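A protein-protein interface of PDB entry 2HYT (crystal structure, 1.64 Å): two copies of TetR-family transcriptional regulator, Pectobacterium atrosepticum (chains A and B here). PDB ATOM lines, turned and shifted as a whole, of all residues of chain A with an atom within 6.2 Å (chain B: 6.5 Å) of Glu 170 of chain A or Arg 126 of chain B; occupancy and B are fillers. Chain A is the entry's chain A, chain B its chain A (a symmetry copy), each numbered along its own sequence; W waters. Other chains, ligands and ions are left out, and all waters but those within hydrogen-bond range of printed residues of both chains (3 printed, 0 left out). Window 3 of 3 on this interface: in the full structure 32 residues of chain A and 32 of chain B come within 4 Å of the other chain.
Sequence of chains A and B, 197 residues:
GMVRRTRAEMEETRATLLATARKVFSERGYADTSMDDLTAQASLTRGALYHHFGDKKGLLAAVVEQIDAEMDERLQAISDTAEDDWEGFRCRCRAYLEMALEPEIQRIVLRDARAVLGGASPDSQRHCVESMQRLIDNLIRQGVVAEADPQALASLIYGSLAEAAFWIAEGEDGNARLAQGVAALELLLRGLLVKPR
NH1 of Arg 114 of chain A is in salt-bridge range of OE2 of Glu 170 of chain A (2.8 Å).
O of Trp 167 of chain A is in hydrogen-bond range of NH1 of Arg 177 of chain A (2.9 Å).
OE1 of Glu 170 of chain A lies within salt-bridge range of NH1 of Arg 177 of chain A (3.9 Å).
OD1 of Asp 123 of chain B lies within salt-bridge range of NH2 of Arg 126 of chain B (2.8 Å).
Water W3 bridges NE of Arg 114 of chain A (2.9 Å) and NE2 of Gln 125 of chain B (3.0 Å).
Water W1 bridges the side-chain carboxylate of Glu 163 of chain A and the side-chain amide oxygen of Gln 125 of chain B.
Water W2 lies within hydrogen-bond range of the side-chain amide oxygen (OE1) of Gln 151 of chain B and the guanidinium group (NH2) of Arg 177 of chain A.
Of the 13 printed residues of chain A, 5 touch a printed residue of chain B.
Hydrophobic or aromatic side chains of chain A that line the printed part of chain B: Trp 167.
Of the 13 printed residues of chain B, 5 touch a printed residue of chain A.
Among the printed residues, 8 pairs touch across the chains.
Among the printed residues, Asp or Glu carboxylates within 4 Å of a Lys or Arg side-chain nitrogen of the other chain: Glu 170 of chain A with Arg 126 of chain B (2.9 Å).
Arg 114 of chain A touches Pro 122 of chain B.
Arg 114 of chain A touches Arg 126 of chain B.
Glu 163 of chain A touches Tyr 158 of chain B.
Gln 151 of chain B touches Arg 177 of chain A.
Arg 111 of chain A touches none of the printed residues of chain B.
Of the printed residues of chain B, Trp 167 of chain A touches Gln 151 (2.9 Å).
Of chain B, only Arg 126 (2.9 Å) comes within 4 Å of Glu 170 of chain A.
Printed residues of chain B within 4 Å of Arg 177 of chain A: Gln 151.
Asp 123 of chain B touches none of the printed residues of chain A.
Arg 126 of chain B touches just these residues of chain A: Arg 114 (3.9 Å) and Glu 170 (2.9 Å).
Printed residues of chain A within 4 Å of Tyr 158 of chain B: Glu 163.
The nearest residue of chain B that does not touch Glu 170 of chain A is Pro 122 of chain B (5.2 Å).
The nearest residue of chain A that does not touch Arg 126 of chain B is Glu 163 of chain A (5.7 Å).
The nearest printed residue of chain A that does not touch Gln 151 of chain B is Glu 170 of chain A (6.1 Å).
The side-chain amide oxygen (OE1) of Gln 125 of chain B sits at hydrogen-bond distance from the guanidinium group (NH2) of Arg 114 of chain A (3.0 Å).
The side-chain carboxylate (OE2) of Glu 163 of chain A sits close to the side-chain amide oxygen (OE1) of Gln 125 of chain B, 2.6 Å away.
The side-chain amide oxygen of Gln 151 of chain B sits at hydrogen-bond distance from the indole nitrogen of Trp 167 of chain A (2.9 Å).
The side-chain carboxylate of Glu 170 of chain A is in salt-bridge range of the guanidinium group of Arg 126 of chain B (2.9 Å).
No position is printed for both chains.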
ATOM      1  N   ARG A 111      -4.562   5.678  16.374  1.00  0.00           N
ATOM      2  CA  ARG A 111      -4.616   4.426  15.616  1.00  0.00           C
ATOM      3  C   ARG A 111      -3.782   4.576  14.314  1.00  0.00           C
ATOM      4  O   ARG A 111      -2.774   3.891  14.092  1.00  0.00           O
ATOM      5  CB  ARG A 111      -6.067   4.032  15.364  1.00  0.00           C
ATOM      6  CG  ARG A 111      -6.757   3.591  16.664  1.00  0.00           C
ATOM      7  CD  ARG A 111      -8.157   3.168  16.382  1.00  0.00           C
ATOM      8  NE  ARG A 111      -8.880   2.874  17.612  1.00  0.00           N
ATOM      9  CZ  ARG A 111     -10.196   2.697  17.686  1.00  0.00           C
ATOM     10  NH1 ARG A 111     -10.951   2.737  16.590  1.00  0.00           N
ATOM     11  NH2 ARG A 111     -10.759   2.474  18.865  1.00  0.00           N
ATOM     12  N   ARG A 114      -0.238   6.221  14.725  1.00  0.00           N
ATOM     13  CA  ARG A 114       0.501   5.210  15.494  1.00  0.00           C
ATOM     14  C   ARG A 114       1.056   4.114  14.601  1.00  0.00           C
ATOM     15  O   ARG A 114       2.263   3.830  14.642  1.00  0.00           O
ATOM     16  CB  ARG A 114      -0.408   4.581  16.565  1.00  0.00           C
ATOM     17  CG  ARG A 114       0.384   3.914  17.639  1.00  0.00           C
ATOM     18  CD  ARG A 114      -0.456   3.029  18.511  1.00  0.00           C
ATOM     19  NE  ARG A 114       0.354   2.608  19.643  1.00  0.00           N
ATOM     20  CZ  ARG A 114      -0.095   1.796  20.604  1.00  0.00           C
ATOM     21  NH1 ARG A 114      -1.315   1.303  20.547  1.00  0.00           N
ATOM     22  NH2 ARG A 114       0.696   1.473  21.593  1.00  0.00           N
ATOM     23  N   GLU A 163       0.978   7.171  26.652  1.00  0.00           N
ATOM     24  CA  GLU A 163       0.788   5.727  26.601  1.00  0.00           C
ATOM     25  C   GLU A 163      -0.632   5.315  27.011  1.00  0.00           C
ATOM     26  O   GLU A 163      -1.248   4.422  26.394  1.00  0.00           O
ATOM     27  CB  GLU A 163       1.801   5.022  27.522  1.00  0.00           C
ATOM     28  CG  GLU A 163       1.993   3.573  27.217  1.00  0.00           C
ATOM     29  CD  GLU A 163       2.625   3.336  25.829  1.00  0.00           C
ATOM     30  OE1 GLU A 163       3.198   4.291  25.215  1.00  0.00           O
ATOM     31  OE2 GLU A 163       2.491   2.193  25.347  1.00  0.00           O
ATOM     32  N   ALA A 165      -3.292   7.081  26.691  1.00  0.00           N
ATOM     33  CA  ALA A 165      -4.186   7.421  25.560  1.00  0.00           C
ATOM     34  C   ALA A 165      -4.185   6.336  24.497  1.00  0.00           C
ATOM     35  O   ALA A 165      -5.249   5.937  24.020  1.00  0.00           O
ATOM     36  CB  ALA A 165      -3.842   8.766  24.976  1.00  0.00           C
ATOM     37  N   PHE A 166      -3.018   5.812  24.146  1.00  0.00           N
ATOM     38  CA  PHE A 166      -2.941   4.664  23.226  1.00  0.00           C
ATOM     39  C   PHE A 166      -3.760   3.496  23.726  1.00  0.00           C
ATOM     40  O   PHE A 166      -4.531   2.889  22.950  1.00  0.00           O
ATOM     41  CB  PHE A 166      -1.507   4.189  23.041  1.00  0.00           C
ATOM     42  CG  PHE A 166      -0.672   5.063  22.146  1.00  0.00           C
ATOM     43  CD1 PHE A 166      -1.165   5.532  20.925  1.00  0.00           C
ATOM     44  CD2 PHE A 166       0.659   5.315  22.452  1.00  0.00           C
ATOM     45  CE1 PHE A 166      -0.353   6.304  20.094  1.00  0.00           C
ATOM     46  CE2 PHE A 166       1.452   6.104  21.618  1.00  0.00           C
ATOM     47  CZ  PHE A 166       0.935   6.564  20.425  1.00  0.00           C
ATOM     48  N   TRP A 167      -3.602   3.211  25.005  1.00  0.00           N
ATOM     49  CA  TRP A 167      -4.244   2.081  25.666  1.00  0.00           C
ATOM     50  C   TRP A 167      -5.752   2.293  25.602  1.00  0.00           C
ATOM     51  O   TRP A 167      -6.516   1.407  25.188  1.00  0.00           O
ATOM     52  CB  TRP A 167      -3.735   1.950  27.097  1.00  0.00           C
ATOM     53  CG  TRP A 167      -4.373   0.868  27.846  1.00  0.00           C
ATOM     54  CD1 TRP A 167      -4.195  -0.478  27.672  1.00  0.00           C
ATOM     55  CD2 TRP A 167      -5.346   1.009  28.898  1.00  0.00           C
ATOM     56  NE1 TRP A 167      -4.964  -1.174  28.559  1.00  0.00           N
ATOM     57  CE2 TRP A 167      -5.685  -0.287  29.320  1.00  0.00           C
ATOM     58  CE3 TRP A 167      -5.933   2.100  29.539  1.00  0.00           C
ATOM     59  CZ2 TRP A 167      -6.595  -0.516  30.317  1.00  0.00           C
ATOM     60  CZ3 TRP A 167      -6.841   1.859  30.550  1.00  0.00           C
ATOM     61  CH2 TRP A 167      -7.194   0.572  30.893  1.00  0.00           C
ATOM     62  N   ILE A 168      -6.205   3.489  25.928  1.00  0.00           N
ATOM     63  CA  ILE A 168      -7.655   3.750  25.890  1.00  0.00           C
ATOM     64  C   ILE A 168      -8.181   3.554  24.464  1.00  0.00           C
ATOM     65  O   ILE A 168      -9.270   2.985  24.268  1.00  0.00           O
ATOM     66  CB  ILE A 168      -7.971   5.166  26.390  1.00  0.00           C
ATOM     67  CG1 ILE A 168      -7.702   5.271  27.881  1.00  0.00           C
ATOM     68  CG2 ILE A 168      -9.398   5.564  26.069  1.00  0.00           C
ATOM     69  CD1 ILE A 168      -7.523   6.695  28.443  1.00  0.00           C
ATOM     70  N   ALA A 169      -7.409   3.992  23.480  1.00  0.00           N
ATOM     71  CA  ALA A 169      -7.811   3.932  22.069  1.00  0.00           C
ATOM     72  C   ALA A 169      -7.743   2.505  21.489  1.00  0.00           C
ATOM     73  O   ALA A 169      -8.313   2.273  20.430  1.00  0.00           O
ATOM     74  CB  ALA A 169      -6.991   4.947  21.232  1.00  0.00           C
ATOM     75  N   GLU A 170      -7.073   1.575  22.188  1.00  0.00           N
ATOM     76  CA  GLU A 170      -6.981   0.125  21.826  1.00  0.00           C
ATOM     77  C   GLU A 170      -8.225  -0.668  22.243  1.00  0.00           C
ATOM     78  O   GLU A 170      -8.474  -1.768  21.715  1.00  0.00           O
ATOM     79  CB  GLU A 170      -5.824  -0.555  22.562  1.00  0.00           C
ATOM     80  CG  GLU A 170      -4.473  -0.342  21.957  1.00  0.00           C
ATOM     81  CD  GLU A 170      -3.315  -0.773  22.856  1.00  0.00           C
ATOM     82  OE1 GLU A 170      -3.497  -1.208  24.016  1.00  0.00           O
ATOM     83  OE2 GLU A 170      -2.189  -0.663  22.388  1.00  0.00           O
ATOM     84  N   GLY A 171      -8.938  -0.175  23.255  1.00  0.00           N
ATOM     85  CA  GLY A 171     -10.095  -0.882  23.772  1.00  0.00           C
ATOM     86  C   GLY A 171     -11.239  -0.942  22.759  1.00  0.00           C
ATOM     87  O   GLY A 171     -11.424  -0.046  21.914  1.00  0.00           O
ATOM     88  N   GLU A 172     -11.994  -2.030  22.823  1.00  0.00           N
ATOM     89  CA  GLU A 172     -13.345  -2.035  22.270  1.00  0.00           C
ATOM     90  C   GLU A 172     -14.202  -1.173  23.223  1.00  0.00           C
ATOM     91  O   GLU A 172     -15.148  -0.514  22.794  1.00  0.00           O
ATOM     92  CB  GLU A 172     -13.885  -3.466  22.180  1.00  0.00           C
ATOM     93  N   ASP A 173     -13.854  -1.171  24.512  1.00  0.00           N
ATOM     94  CA  ASP A 173     -14.568  -0.351  25.481  1.00  0.00           C
ATOM     95  C   ASP A 173     -13.684   0.792  25.969  1.00  0.00           C
ATOM     96  O   ASP A 173     -13.161   0.800  27.090  1.00  0.00           O
ATOM     97  CB  ASP A 173     -15.136  -1.177  26.647  1.00  0.00           C
ATOM     98  CG  ASP A 173     -16.319  -0.501  27.299  1.00  0.00           C
ATOM     99  OD1 ASP A 173     -16.370   0.760  27.268  1.00  0.00           O
ATOM    100  OD2 ASP A 173     -17.212  -1.227  27.802  1.00  0.00           O
ATOM    101  N   ARG A 177     -12.145   1.984  29.743  1.00  0.00           N
ATOM    102  CA  ARG A 177     -10.700   2.217  29.902  1.00  0.00           C
ATOM    103  C   ARG A 177     -10.434   3.658  30.316  1.00  0.00           C
ATOM    104  O   ARG A 177      -9.555   3.921  31.154  1.00  0.00           O
ATOM    105  CB  ARG A 177      -9.946   1.908  28.607  1.00  0.00           C
ATOM    106  CG  ARG A 177      -9.903   0.425  28.334  1.00  0.00           C
ATOM    107  CD  ARG A 177      -8.837   0.071  27.355  1.00  0.00           C
ATOM    108  NE  ARG A 177      -8.767  -1.369  27.239  1.00  0.00           N
ATOM    109  CZ  ARG A 177      -7.866  -2.047  26.538  1.00  0.00           C
ATOM    110  NH1 ARG A 177      -6.957  -1.423  25.849  1.00  0.00           N
ATOM    111  NH2 ARG A 177      -7.897  -3.382  26.510  1.00  0.00           N
ATOM    112  N   SER B 121       7.524  -1.104  18.951  1.00  0.00           N
ATOM    113  CA  SER B 121       6.286  -1.468  18.289  1.00  0.00           C
ATOM    114  C   SER B 121       5.132  -1.469  19.301  1.00  0.00           C
ATOM    115  O   SER B 121       5.368  -1.701  20.465  1.00  0.00           O
ATOM    116  CB  SER B 121       6.386  -2.859  17.662  1.00  0.00           C
ATOM    117  OG  SER B 121       6.638  -3.852  18.629  1.00  0.00           O
ATOM    118  N   PRO B 122       3.889  -1.219  18.846  1.00  0.00           N
ATOM    119  CA  PRO B 122       2.739  -1.419  19.726  1.00  0.00           C
ATOM    120  C   PRO B 122       2.732  -2.799  20.396  1.00  0.00           C
ATOM    121  O   PRO B 122       2.383  -2.917  21.583  1.00  0.00           O
ATOM    122  CB  PRO B 122       1.548  -1.216  18.788  1.00  0.00           C
ATOM    123  CG  PRO B 122       2.072  -0.198  17.783  1.00  0.00           C
ATOM    124  CD  PRO B 122       3.481  -0.644  17.548  1.00  0.00           C
ATOM    125  N   ASP B 123       3.138  -3.842  19.677  1.00  0.00           N
ATOM    126  CA  ASP B 123       3.196  -5.172  20.285  1.00  0.00           C
ATOM    127  C   ASP B 123       4.182  -5.213  21.450  1.00  0.00           C
ATOM    128  O   ASP B 123       3.884  -5.800  22.508  1.00  0.00           O
ATOM    129  CB  ASP B 123       3.617  -6.233  19.272  1.00  0.00           C
ATOM    130  CG  ASP B 123       2.478  -6.725  18.398  1.00  0.00           C
ATOM    131  OD1 ASP B 123       1.280  -6.401  18.637  1.00  0.00           O
ATOM    132  OD2 ASP B 123       2.820  -7.484  17.456  1.00  0.00           O
ATOM    133  N   SER B 124       5.376  -4.639  21.231  1.00  0.00           N
ATOM    134  CA  SER B 124       6.422  -4.594  22.257  1.00  0.00           C
ATOM    135  C   SER B 124       5.944  -3.810  23.477  1.00  0.00           C
ATOM    136  O   SER B 124       6.195  -4.187  24.625  1.00  0.00           O
ATOM    137  CB  SER B 124       7.700  -3.947  21.722  1.00  0.00           C
ATOM    138  OG  SER B 124       8.662  -3.841  22.754  1.00  0.00           O
ATOM    139  N   GLN B 125       5.260  -2.711  23.214  1.00  0.00           N
ATOM    140  CA  GLN B 125       4.677  -1.902  24.274  1.00  0.00           C
ATOM    141  C   GLN B 125       3.656  -2.710  25.099  1.00  0.00           C
ATOM    142  O   GLN B 125       3.691  -2.718  26.340  1.00  0.00           O
ATOM    143  CB  GLN B 125       3.993  -0.697  23.667  1.00  0.00           C
ATOM    144  CG  GLN B 125       4.978   0.277  23.000  1.00  0.00           C
ATOM    145  CD  GLN B 125       4.251   1.409  22.323  1.00  0.00           C
ATOM    146  OE1 GLN B 125       3.388   2.022  22.906  1.00  0.00           O
ATOM    147  NE2 GLN B 125       4.604   1.689  21.103  1.00  0.00           N
ATOM    148  N   ARG B 126       2.768  -3.430  24.415  1.00  0.00           N
ATOM    149  CA  ARG B 126       1.748  -4.206  25.119  1.00  0.00           C
ATOM    150  C   ARG B 126       2.424  -5.283  25.942  1.00  0.00           C
ATOM    151  O   ARG B 126       1.987  -5.581  27.059  1.00  0.00           O
ATOM    152  CB  ARG B 126       0.752  -4.792  24.118  1.00  0.00           C
ATOM    153  CG  ARG B 126      -0.214  -3.708  23.615  1.00  0.00           C
ATOM    154  CD  ARG B 126      -1.363  -4.219  22.753  1.00  0.00           C
ATOM    155  NE  ARG B 126      -0.908  -4.632  21.425  1.00  0.00           N
ATOM    156  CZ  ARG B 126      -0.923  -3.856  20.341  1.00  0.00           C
ATOM    157  NH1 ARG B 126      -1.363  -2.608  20.389  1.00  0.00           N
ATOM    158  NH2 ARG B 126      -0.476  -4.334  19.195  1.00  0.00           N
ATOM    159  N   HIS B 127       3.482  -5.874  25.407  1.00  0.00           N
ATOM    160  CA  HIS B 127       4.241  -6.857  26.156  1.00  0.00           C
ATOM    161  C   HIS B 127       4.864  -6.303  27.475  1.00  0.00           C
ATOM    162  O   HIS B 127       4.804  -6.930  28.527  1.00  0.00           O
ATOM    163  CB  HIS B 127       5.331  -7.423  25.257  1.00  0.00           C
ATOM    164  CG  HIS B 127       5.935  -8.679  25.777  1.00  0.00           C
ATOM    165  ND1 HIS B 127       7.180  -8.718  26.366  1.00  0.00           N
ATOM    166  CD2 HIS B 127       5.457  -9.947  25.813  1.00  0.00           C
ATOM    167  CE1 HIS B 127       7.446  -9.959  26.739  1.00  0.00           C
ATOM    168  NE2 HIS B 127       6.422 -10.725  26.409  1.00  0.00           N
ATOM    169  N   CYS B 128       5.451  -5.121  27.397  1.00  0.00           N
ATOM    170  CA  CYS B 128       6.059  -4.486  28.546  1.00  0.00           C
ATOM    171  C   CYS B 128       4.961  -4.173  29.559  1.00  0.00           C
ATOM    172  O   CYS B 128       5.155  -4.304  30.785  1.00  0.00           O
ATOM    173  CB  CYS B 128       6.753  -3.185  28.139  1.00  0.00           C
ATOM    174  SG  CYS B 128       8.231  -3.361  27.161  1.00  0.00           S
ATOM    175  N   VAL B 129       3.834  -3.705  29.038  1.00  0.00           N
ATOM    176  CA  VAL B 129       2.723  -3.369  29.935  1.00  0.00           C
ATOM    177  C   VAL B 129       2.215  -4.616  30.662  1.00  0.00           C
ATOM    178  O   VAL B 129       1.924  -4.547  31.851  1.00  0.00           O
ATOM    179  CB  VAL B 129       1.616  -2.639  29.184  1.00  0.00           C
ATOM    180  CG1 VAL B 129       0.336  -2.555  29.989  1.00  0.00           C
ATOM    181  CG2 VAL B 129       2.135  -1.235  28.745  1.00  0.00           C
ATOM    182  N   GLU B 130       2.090  -5.739  29.960  1.00  0.00           N
ATOM    183  CA  GLU B 130       1.617  -6.964  30.593  1.00  0.00           C
ATOM    184  C   GLU B 130       2.556  -7.412  31.723  1.00  0.00           C
ATOM    185  O   GLU B 130       2.094  -7.860  32.763  1.00  0.00           O
ATOM    186  CB  GLU B 130       1.424  -8.047  29.540  1.00  0.00           C
ATOM    187  CG  GLU B 130       0.219  -7.750  28.676  1.00  0.00           C
ATOM    188  CD  GLU B 130       0.161  -8.537  27.379  1.00  0.00           C
ATOM    189  OE1 GLU B 130       1.097  -9.332  27.112  1.00  0.00           O
ATOM    190  OE2 GLU B 130      -0.822  -8.338  26.619  1.00  0.00           O
ATOM    191  N   SER B 131       3.861  -7.262  31.519  1.00  0.00           N
ATOM    192  CA  SER B 131       4.842  -7.624  32.544  1.00  0.00           C
ATOM    193  C   SER B 131       4.676  -6.721  33.755  1.00  0.00           C
ATOM    194  O   SER B 131       4.595  -7.184  34.888  1.00  0.00           O
ATOM    195  CB  SER B 131       6.248  -7.521  32.012  1.00  0.00           C
ATOM    196  OG  SER B 131       7.187  -7.889  33.003  1.00  0.00           O
ATOM    197  N   GLN B 151      -3.865  -2.986  34.580  1.00  0.00           N
ATOM    198  CA  GLN B 151      -3.421  -2.735  33.213  1.00  0.00           C
ATOM    199  C   GLN B 151      -3.318  -1.226  32.930  1.00  0.00           C
ATOM    200  O   GLN B 151      -2.377  -0.764  32.280  1.00  0.00           O
ATOM    201  CB  GLN B 151      -4.295  -3.391  32.177  1.00  0.00           C
ATOM    202  CG  GLN B 151      -3.583  -3.501  30.826  1.00  0.00           C
ATOM    203  CD  GLN B 151      -4.314  -4.407  29.881  1.00  0.00           C
ATOM    204  OE1 GLN B 151      -5.200  -3.967  29.174  1.00  0.00           O
ATOM    205  NE2 GLN B 151      -3.975  -5.704  29.895  1.00  0.00           N
ATOM    206  N   TYR B 158       4.706   2.375  32.578  1.00  0.00           N
ATOM    207  CA  TYR B 158       5.537   2.034  31.422  1.00  0.00           C
ATOM    208  C   TYR B 158       5.735   3.283  30.535  1.00  0.00           C
ATOM    209  O   TYR B 158       6.869   3.611  30.118  1.00  0.00           O
ATOM    210  CB  TYR B 158       4.971   0.833  30.624  1.00  0.00           C
ATOM    211  CG  TYR B 158       5.640   0.770  29.257  1.00  0.00           C
ATOM    212  CD1 TYR B 158       6.958   0.323  29.147  1.00  0.00           C
ATOM    213  CD2 TYR B 158       5.025   1.205  28.135  1.00  0.00           C
ATOM    214  CE1 TYR B 158       7.613   0.324  27.934  1.00  0.00           C
ATOM    215  CE2 TYR B 158       5.666   1.221  26.915  1.00  0.00           C
ATOM    216  CZ  TYR B 158       6.950   0.725  26.815  1.00  0.00           C
ATOM    217  OH  TYR B 158       7.576   0.721  25.593  1.00  0.00           O
HETATM  218  O   HOH W   1       4.755   4.770  22.682  1.00  0.00           O
HETATM  219  O   HOH W   2      -5.443  -5.527  26.445  1.00  0.00           O
HETATM  220  O   HOH W   3       3.014   3.706  19.574  1.00  0.00           O
